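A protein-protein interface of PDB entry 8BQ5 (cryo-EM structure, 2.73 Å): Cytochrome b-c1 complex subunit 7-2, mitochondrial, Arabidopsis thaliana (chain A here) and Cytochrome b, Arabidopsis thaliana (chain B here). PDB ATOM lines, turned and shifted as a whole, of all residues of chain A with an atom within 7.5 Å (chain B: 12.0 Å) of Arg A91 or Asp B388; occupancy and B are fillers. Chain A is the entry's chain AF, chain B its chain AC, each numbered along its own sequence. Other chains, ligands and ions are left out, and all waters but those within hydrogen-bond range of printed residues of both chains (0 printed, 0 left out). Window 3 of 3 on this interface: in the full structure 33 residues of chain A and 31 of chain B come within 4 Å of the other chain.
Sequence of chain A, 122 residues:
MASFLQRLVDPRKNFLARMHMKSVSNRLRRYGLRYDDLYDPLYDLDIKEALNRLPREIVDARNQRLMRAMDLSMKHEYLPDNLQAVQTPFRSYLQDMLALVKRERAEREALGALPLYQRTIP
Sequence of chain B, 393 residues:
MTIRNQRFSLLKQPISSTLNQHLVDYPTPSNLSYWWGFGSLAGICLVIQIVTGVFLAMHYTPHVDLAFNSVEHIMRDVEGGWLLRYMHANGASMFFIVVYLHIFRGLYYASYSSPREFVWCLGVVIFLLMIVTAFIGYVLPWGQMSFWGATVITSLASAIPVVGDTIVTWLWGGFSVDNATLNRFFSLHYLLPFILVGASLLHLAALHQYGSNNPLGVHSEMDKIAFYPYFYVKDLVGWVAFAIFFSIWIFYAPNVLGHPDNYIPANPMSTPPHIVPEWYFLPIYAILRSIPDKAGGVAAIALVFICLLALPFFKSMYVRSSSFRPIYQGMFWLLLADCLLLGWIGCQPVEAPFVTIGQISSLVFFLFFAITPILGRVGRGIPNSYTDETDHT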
ATOM      1  N   MET A  21       8.571 -14.427 -28.082  1.00  0.00           N
ATOM      2  CA  MET A  21       7.251 -14.119 -27.543  1.00  0.00           C
ATOM      3  C   MET A  21       6.255 -13.828 -28.656  1.00  0.00           C
ATOM      4  O   MET A  21       5.093 -14.242 -28.584  1.00  0.00           O
ATOM      5  CB  MET A  21       7.339 -12.937 -26.577  1.00  0.00           C
ATOM      6  CG  MET A  21       6.002 -12.517 -25.991  1.00  0.00           C
ATOM      7  SD  MET A  21       6.132 -11.112 -24.870  1.00  0.00           S
ATOM      8  CE  MET A  21       6.487  -9.788 -26.022  1.00  0.00           C
ATOM      9  N   ARG A  29      -2.844 -17.204 -30.781  1.00  0.00           N
ATOM     10  CA  ARG A  29      -3.942 -16.342 -31.207  1.00  0.00           C
ATOM     11  C   ARG A  29      -4.768 -16.991 -32.310  1.00  0.00           C
ATOM     12  O   ARG A  29      -5.982 -16.773 -32.398  1.00  0.00           O
ATOM     13  CB  ARG A  29      -3.382 -15.002 -31.673  1.00  0.00           C
ATOM     14  CG  ARG A  29      -4.417 -13.958 -31.983  1.00  0.00           C
ATOM     15  CD  ARG A  29      -3.744 -12.643 -32.309  1.00  0.00           C
ATOM     16  NE  ARG A  29      -3.035 -12.110 -31.154  1.00  0.00           N
ATOM     17  CZ  ARG A  29      -3.515 -11.167 -30.356  1.00  0.00           C
ATOM     18  NH1 ARG A  29      -4.719 -10.653 -30.542  1.00  0.00           N
ATOM     19  NH2 ARG A  29      -2.771 -10.733 -29.342  1.00  0.00           N
ATOM     20  N   ARG A  34      -5.095 -19.393 -24.643  1.00  0.00           N
ATOM     21  CA  ARG A  34      -4.167 -18.696 -23.773  1.00  0.00           C
ATOM     22  C   ARG A  34      -3.021 -19.632 -23.418  1.00  0.00           C
ATOM     23  O   ARG A  34      -3.143 -20.854 -23.524  1.00  0.00           O
ATOM     24  CB  ARG A  34      -4.876 -18.203 -22.512  1.00  0.00           C
ATOM     25  CG  ARG A  34      -5.790 -17.027 -22.782  1.00  0.00           C
ATOM     26  CD  ARG A  34      -6.187 -16.311 -21.513  1.00  0.00           C
ATOM     27  NE  ARG A  34      -7.540 -15.781 -21.603  1.00  0.00           N
ATOM     28  CZ  ARG A  34      -8.212 -15.265 -20.584  1.00  0.00           C
ATOM     29  NH1 ARG A  34      -7.683 -15.194 -19.374  1.00  0.00           N
ATOM     30  NH2 ARG A  34      -9.443 -14.805 -20.784  1.00  0.00           N
ATOM     31  N   TYR A  35      -1.893 -19.047 -23.015  1.00  0.00           N
ATOM     32  CA  TYR A  35      -0.729 -19.867 -22.699  1.00  0.00           C
ATOM     33  C   TYR A  35      -1.009 -20.790 -21.520  1.00  0.00           C
ATOM     34  O   TYR A  35      -0.484 -21.909 -21.459  1.00  0.00           O
ATOM     35  CB  TYR A  35       0.483 -18.987 -22.413  1.00  0.00           C
ATOM     36  CG  TYR A  35       1.778 -19.759 -22.417  1.00  0.00           C
ATOM     37  CD1 TYR A  35       2.396 -20.104 -23.610  1.00  0.00           C
ATOM     38  CD2 TYR A  35       2.374 -20.158 -21.230  1.00  0.00           C
ATOM     39  CE1 TYR A  35       3.576 -20.815 -23.621  1.00  0.00           C
ATOM     40  CE2 TYR A  35       3.554 -20.869 -21.232  1.00  0.00           C
ATOM     41  CZ  TYR A  35       4.151 -21.195 -22.429  1.00  0.00           C
ATOM     42  OH  TYR A  35       5.328 -21.904 -22.436  1.00  0.00           O
ATOM     43  N   ASP A  36      -1.834 -20.340 -20.575  1.00  0.00           N
ATOM     44  CA  ASP A  36      -2.188 -21.186 -19.443  1.00  0.00           C
ATOM     45  C   ASP A  36      -3.070 -22.352 -19.866  1.00  0.00           C
ATOM     46  O   ASP A  36      -3.102 -23.381 -19.182  1.00  0.00           O
ATOM     47  CB  ASP A  36      -2.881 -20.356 -18.368  1.00  0.00           C
ATOM     48  CG  ASP A  36      -1.912 -19.510 -17.579  1.00  0.00           C
ATOM     49  OD1 ASP A  36      -0.696 -19.601 -17.844  1.00  0.00           O
ATOM     50  OD2 ASP A  36      -2.365 -18.749 -16.701  1.00  0.00           O
ATOM     51  N   ASP A  37      -3.793 -22.211 -20.979  1.00  0.00           N
ATOM     52  CA  ASP A  37      -4.595 -23.316 -21.490  1.00  0.00           C
ATOM     53  C   ASP A  37      -3.740 -24.502 -21.913  1.00  0.00           C
ATOM     54  O   ASP A  37      -4.242 -25.629 -21.953  1.00  0.00           O
ATOM     55  CB  ASP A  37      -5.452 -22.853 -22.669  1.00  0.00           C
ATOM     56  CG  ASP A  37      -6.501 -21.838 -22.266  1.00  0.00           C
ATOM     57  OD1 ASP A  37      -6.933 -21.857 -21.095  1.00  0.00           O
ATOM     58  OD2 ASP A  37      -6.900 -21.025 -23.125  1.00  0.00           O
ATOM     59  N   ARG A  65     -12.547 -22.479 -24.242  1.00  0.00           N
ATOM     60  CA  ARG A  65     -11.467 -22.147 -25.164  1.00  0.00           C
ATOM     61  C   ARG A  65     -10.794 -23.405 -25.698  1.00  0.00           C
ATOM     62  O   ARG A  65     -10.400 -23.459 -26.868  1.00  0.00           O
ATOM     63  CB  ARG A  65     -10.452 -21.231 -24.479  1.00  0.00           C
ATOM     64  CG  ARG A  65     -10.839 -19.762 -24.532  1.00  0.00           C
ATOM     65  CD  ARG A  65      -9.729 -18.847 -24.037  1.00  0.00           C
ATOM     66  NE  ARG A  65      -9.087 -19.345 -22.827  1.00  0.00           N
ATOM     67  CZ  ARG A  65      -9.438 -19.001 -21.596  1.00  0.00           C
ATOM     68  NH1 ARG A  65     -10.440 -18.168 -21.370  1.00  0.00           N
ATOM     69  NH2 ARG A  65      -8.769 -19.507 -20.565  1.00  0.00           N
ATOM     70  N   VAL A  86      -9.208  -9.701 -30.827  1.00  0.00           N
ATOM     71  CA  VAL A  86      -9.632  -9.511 -29.445  1.00  0.00           C
ATOM     72  C   VAL A  86      -9.087 -10.598 -28.529  1.00  0.00           C
ATOM     73  O   VAL A  86      -9.498 -10.689 -27.369  1.00  0.00           O
ATOM     74  CB  VAL A  86     -11.163  -9.421 -29.336  1.00  0.00           C
ATOM     75  CG1 VAL A  86     -11.654  -8.104 -29.912  1.00  0.00           C
ATOM     76  CG2 VAL A  86     -11.822 -10.591 -30.041  1.00  0.00           C
ATOM     77  N   GLN A  87      -8.168 -11.426 -29.018  1.00  0.00           N
ATOM     78  CA  GLN A  87      -7.578 -12.471 -28.197  1.00  0.00           C
ATOM     79  C   GLN A  87      -6.516 -11.894 -27.268  1.00  0.00           C
ATOM     80  O   GLN A  87      -5.881 -10.878 -27.566  1.00  0.00           O
ATOM     81  CB  GLN A  87      -6.964 -13.562 -29.075  1.00  0.00           C
ATOM     82  CG  GLN A  87      -7.974 -14.340 -29.899  1.00  0.00           C
ATOM     83  CD  GLN A  87      -9.174 -14.782 -29.088  1.00  0.00           C
ATOM     84  OE1 GLN A  87      -9.037 -15.489 -28.090  1.00  0.00           O
ATOM     85  NE2 GLN A  87     -10.361 -14.367 -29.512  1.00  0.00           N
ATOM     86  N   THR A  88      -6.331 -12.556 -26.126  1.00  0.00           N
ATOM     87  CA  THR A  88      -5.340 -12.167 -25.120  1.00  0.00           C
ATOM     88  C   THR A  88      -4.498 -13.393 -24.797  1.00  0.00           C
ATOM     89  O   THR A  88      -4.724 -14.065 -23.781  1.00  0.00           O
ATOM     90  CB  THR A  88      -6.006 -11.611 -23.861  1.00  0.00           C
ATOM     91  OG1 THR A  88      -6.940 -12.571 -23.350  1.00  0.00           O
ATOM     92  CG2 THR A  88      -6.739 -10.319 -24.170  1.00  0.00           C
ATOM     93  N   PRO A  89      -3.514 -13.712 -25.640  1.00  0.00           N
ATOM     94  CA  PRO A  89      -2.786 -14.983 -25.475  1.00  0.00           C
ATOM     95  C   PRO A  89      -2.064 -15.123 -24.147  1.00  0.00           C
ATOM     96  O   PRO A  89      -1.934 -16.247 -23.646  1.00  0.00           O
ATOM     97  CB  PRO A  89      -1.795 -14.974 -26.649  1.00  0.00           C
ATOM     98  CG  PRO A  89      -2.339 -13.979 -27.616  1.00  0.00           C
ATOM     99  CD  PRO A  89      -3.034 -12.944 -26.798  1.00  0.00           C
ATOM    100  N   PHE A  90      -1.588 -14.028 -23.556  1.00  0.00           N
ATOM    101  CA  PHE A  90      -0.765 -14.104 -22.356  1.00  0.00           C
ATOM    102  C   PHE A  90      -1.454 -13.520 -21.127  1.00  0.00           C
ATOM    103  O   PHE A  90      -0.783 -13.210 -20.138  1.00  0.00           O
ATOM    104  CB  PHE A  90       0.579 -13.417 -22.596  1.00  0.00           C
ATOM    105  CG  PHE A  90       1.551 -14.262 -23.363  1.00  0.00           C
ATOM    106  CD1 PHE A  90       2.059 -15.427 -22.814  1.00  0.00           C
ATOM    107  CD2 PHE A  90       1.944 -13.903 -24.640  1.00  0.00           C
ATOM    108  CE1 PHE A  90       2.947 -16.212 -23.520  1.00  0.00           C
ATOM    109  CE2 PHE A  90       2.832 -14.685 -25.351  1.00  0.00           C
ATOM    110  CZ  PHE A  90       3.334 -15.840 -24.790  1.00  0.00           C
ATOM    111  N   ARG A  91      -2.775 -13.369 -21.164  1.00  0.00           N
ATOM    112  CA  ARG A  91      -3.523 -12.991 -19.972  1.00  0.00           C
ATOM    113  C   ARG A  91      -3.569 -14.188 -19.030  1.00  0.00           C
ATOM    114  O   ARG A  91      -4.178 -15.213 -19.348  1.00  0.00           O
ATOM    115  CB  ARG A  91      -4.930 -12.527 -20.338  1.00  0.00           C
ATOM    116  CG  ARG A  91      -5.715 -11.965 -19.165  1.00  0.00           C
ATOM    117  CD  ARG A  91      -6.917 -11.165 -19.635  1.00  0.00           C
ATOM    118  NE  ARG A  91      -6.530  -9.886 -20.218  1.00  0.00           N
ATOM    119  CZ  ARG A  91      -7.363  -9.064 -20.840  1.00  0.00           C
ATOM    120  NH1 ARG A  91      -8.643  -9.360 -20.987  1.00  0.00           N
ATOM    121  NH2 ARG A  91      -6.900  -7.918 -21.327  1.00  0.00           N
ATOM    122  N   SER A  92      -2.931 -14.054 -17.875  1.00  0.00           N
ATOM    123  CA  SER A  92      -2.665 -15.187 -17.000  1.00  0.00           C
ATOM    124  C   SER A  92      -3.790 -15.395 -15.993  1.00  0.00           C
ATOM    125  O   SER A  92      -4.389 -14.434 -15.504  1.00  0.00           O
ATOM    126  CB  SER A  92      -1.338 -14.978 -16.269  1.00  0.00           C
ATOM    127  OG  SER A  92      -1.359 -13.786 -15.504  1.00  0.00           O
ATOM    128  N   TYR A  93      -4.082 -16.665 -15.701  1.00  0.00           N
ATOM    129  CA  TYR A  93      -5.036 -17.021 -14.658  1.00  0.00           C
ATOM    130  C   TYR A  93      -4.581 -18.167 -13.765  1.00  0.00           C
ATOM    131  O   TYR A  93      -5.242 -18.431 -12.755  1.00  0.00           O
ATOM    132  CB  TYR A  93      -6.401 -17.381 -15.271  1.00  0.00           C
ATOM    133  CG  TYR A  93      -6.399 -18.612 -16.155  1.00  0.00           C
ATOM    134  CD1 TYR A  93      -6.524 -19.886 -15.613  1.00  0.00           C
ATOM    135  CD2 TYR A  93      -6.279 -18.499 -17.533  1.00  0.00           C
ATOM    136  CE1 TYR A  93      -6.521 -21.007 -16.414  1.00  0.00           C
ATOM    137  CE2 TYR A  93      -6.278 -19.616 -18.343  1.00  0.00           C
ATOM    138  CZ  TYR A  93      -6.398 -20.867 -17.777  1.00  0.00           C
ATOM    139  OH  TYR A  93      -6.396 -21.984 -18.578  1.00  0.00           O
ATOM    140  N   LEU A  94      -3.486 -18.849 -14.092  1.00  0.00           N
ATOM    141  CA  LEU A  94      -3.112 -20.096 -13.438  1.00  0.00           C
ATOM    142  C   LEU A  94      -1.756 -20.060 -12.748  1.00  0.00           C
ATOM    143  O   LEU A  94      -1.555 -20.803 -11.786  1.00  0.00           O
ATOM    144  CB  LEU A  94      -3.115 -21.242 -14.463  1.00  0.00           C
ATOM    145  CG  LEU A  94      -2.791 -22.667 -14.012  1.00  0.00           C
ATOM    146  CD1 LEU A  94      -3.883 -23.213 -13.109  1.00  0.00           C
ATOM    147  CD2 LEU A  94      -2.592 -23.563 -15.221  1.00  0.00           C
ATOM    148  N   GLY B 381      10.000 -20.655 -17.015  1.00  0.00           N
ATOM    149  CA  GLY B 381       9.763 -19.263 -16.712  1.00  0.00           C
ATOM    150  C   GLY B 381       9.184 -18.446 -17.839  1.00  0.00           C
ATOM    151  O   GLY B 381       9.158 -17.216 -17.749  1.00  0.00           O
ATOM    152  N   ILE B 382       8.735 -19.094 -18.915  1.00  0.00           N
ATOM    153  CA  ILE B 382       8.105 -18.360 -20.014  1.00  0.00           C
ATOM    154  C   ILE B 382       6.830 -17.645 -19.576  1.00  0.00           C
ATOM    155  O   ILE B 382       6.684 -16.450 -19.883  1.00  0.00           O
ATOM    156  CB  ILE B 382       7.882 -19.294 -21.216  1.00  0.00           C
ATOM    157  CG1 ILE B 382       9.158 -19.401 -22.050  1.00  0.00           C
ATOM    158  CG2 ILE B 382       6.730 -18.799 -22.077  1.00  0.00           C
ATOM    159  CD1 ILE B 382       8.975 -20.166 -23.337  1.00  0.00           C
ATOM    160  N   PRO B 383       5.881 -18.285 -18.882  1.00  0.00           N
ATOM    161  CA  PRO B 383       4.663 -17.558 -18.485  1.00  0.00           C
ATOM    162  C   PRO B 383       4.918 -16.387 -17.552  1.00  0.00           C
ATOM    163  O   PRO B 383       4.120 -15.444 -17.538  1.00  0.00           O
ATOM    164  CB  PRO B 383       3.811 -18.641 -17.807  1.00  0.00           C
ATOM    165  CG  PRO B 383       4.781 -19.691 -17.404  1.00  0.00           C
ATOM    166  CD  PRO B 383       5.800 -19.705 -18.491  1.00  0.00           C
ATOM    167  N   ASN B 384       5.995 -16.415 -16.769  1.00  0.00           N
ATOM    168  CA  ASN B 384       6.304 -15.324 -15.855  1.00  0.00           C
ATOM    169  C   ASN B 384       7.076 -14.188 -16.511  1.00  0.00           C
ATOM    170  O   ASN B 384       7.219 -13.124 -15.900  1.00  0.00           O
ATOM    171  CB  ASN B 384       7.098 -15.850 -14.655  1.00  0.00           C
ATOM    172  CG  ASN B 384       6.414 -17.015 -13.968  1.00  0.00           C
ATOM    173  OD1 ASN B 384       5.528 -16.826 -13.135  1.00  0.00           O
ATOM    174  ND2 ASN B 384       6.823 -18.229 -14.317  1.00  0.00           N
ATOM    175  N   SER B 385       7.575 -14.381 -17.734  1.00  0.00           N
ATOM    176  CA  SER B 385       8.317 -13.343 -18.433  1.00  0.00           C
ATOM    177  C   SER B 385       7.551 -12.714 -19.585  1.00  0.00           C
ATOM    178  O   SER B 385       7.754 -11.529 -19.865  1.00  0.00           O
ATOM    179  CB  SER B 385       9.644 -13.901 -18.967  1.00  0.00           C
ATOM    180  OG  SER B 385       9.418 -14.907 -19.938  1.00  0.00           O
ATOM    181  N   TYR B 386       6.683 -13.467 -20.252  1.00  0.00           N
ATOM    182  CA  TYR B 386       5.864 -12.968 -21.354  1.00  0.00           C
ATOM    183  C   TYR B 386       4.504 -12.611 -20.758  1.00  0.00           C
ATOM    184  O   TYR B 386       3.605 -13.447 -20.678  1.00  0.00           O
ATOM    185  CB  TYR B 386       5.739 -14.009 -22.466  1.00  0.00           C
ATOM    186  CG  TYR B 386       7.045 -14.359 -23.148  1.00  0.00           C
ATOM    187  CD1 TYR B 386       8.166 -13.549 -23.014  1.00  0.00           C
ATOM    188  CD2 TYR B 386       7.158 -15.512 -23.912  1.00  0.00           C
ATOM    189  CE1 TYR B 386       9.360 -13.875 -23.631  1.00  0.00           C
ATOM    190  CE2 TYR B 386       8.346 -15.845 -24.532  1.00  0.00           C
ATOM    191  CZ  TYR B 386       9.442 -15.025 -24.386  1.00  0.00           C
ATOM    192  OH  TYR B 386      10.626 -15.356 -25.002  1.00  0.00           O
ATOM    193  N   THR B 387       4.366 -11.361 -20.333  1.00  0.00           N
ATOM    194  CA  THR B 387       3.161 -10.908 -19.656  1.00  0.00           C
ATOM    195  C   THR B 387       2.259 -10.138 -20.611  1.00  0.00           C
ATOM    196  O   THR B 387       2.719  -9.521 -21.576  1.00  0.00           O
ATOM    197  CB  THR B 387       3.512 -10.034 -18.452  1.00  0.00           C
ATOM    198  OG1 THR B 387       4.212  -8.864 -18.895  1.00  0.00           O
ATOM    199  CG2 THR B 387       4.384 -10.803 -17.471  1.00  0.00           C
ATOM    200  N   ASP B 388       0.961 -10.186 -20.330  1.00  0.00           N
ATOM    201  CA  ASP B 388      -0.036  -9.523 -21.161  1.00  0.00           C
ATOM    202  C   ASP B 388       0.064  -8.006 -21.040  1.00  0.00           C
ATOM    203  O   ASP B 388       0.282  -7.308 -22.031  1.00  0.00           O
ATOM    204  CB  ASP B 388      -1.440  -9.992 -20.775  1.00  0.00           C
ATOM    205  CG  ASP B 388      -2.523  -9.347 -21.615  1.00  0.00           C
ATOM    206  OD1 ASP B 388      -2.277  -9.088 -22.811  1.00  0.00           O
ATOM    207  OD2 ASP B 388      -3.623  -9.104 -21.078  1.00  0.00           O
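CG of Met A21 touches CG of Tyr B386, 3.5 Å away.
Tyr A35 touches Ile B382 (OH to CG2, 3.4 Å).
Tyr A35 touches Pro B383 (CE2 to CD, 3.7 Å).
O of Tyr B386 touches CD1 of Phe A90, 3.3 Å away.
Of the printed residues of chain B, Met A21 touches Tyr B386.
Printed residues of chain B within 4 Å of Tyr A35: Ile B382 (3.4 Å) and Pro B383 (3.7 Å).
Thr A88 touches none of the printed residues of chain B.
Of the printed residues of chain B, Phe A90 touches Tyr B386 (3.3 Å) and Asp B388 (3.3 Å).
Of chain B, only Asp B388 (3.1 Å) comes within 4 Å of Arg A91.
No residue of chain B comes within 4 Å of Ser A92.
No residue of chain B comes within 4 Å of Tyr A93.
Of the printed residues of chain A, Ile B382 touches Tyr A35.
Printed residues of chain A within 4 Å of Pro B383: Tyr A35.
Ser B385 touches none of the printed residues of chain A.
Asp B388 touches two residues of chain A.
The nearest residue of chain B that does not touch Arg A91 is Thr B387 (6.0 Å).
The nearest residue of chain A that does not touch Asp B388 is Thr A88 (4.4 Å).
Printed residues of chain B that touch a printed residue of chain A: Ile B382, Pro B383, Tyr B386 and Asp B388.
Of the 16 printed residues of chain A, 4 touch a printed residue of chain B.
Hydrophobic or aromatic side chains of chain A that line the printed part of chain B: Met A21, Tyr A35 and Phe A90.
O of Phe A90 lies close to N of Asp B388 (3.5 Å).
NE of Arg A91 lies within salt-bridge range of OD2 of Asp B388.
O of Ile B382 sits at hydrogen-bond distance from OG of Ser B385 (3.1 Å).
The backbone carbonyl oxygen (O) of Pro A89 is in hydrogen-bond range of the backbone NH (N) of Tyr A35 (2.9 Å).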
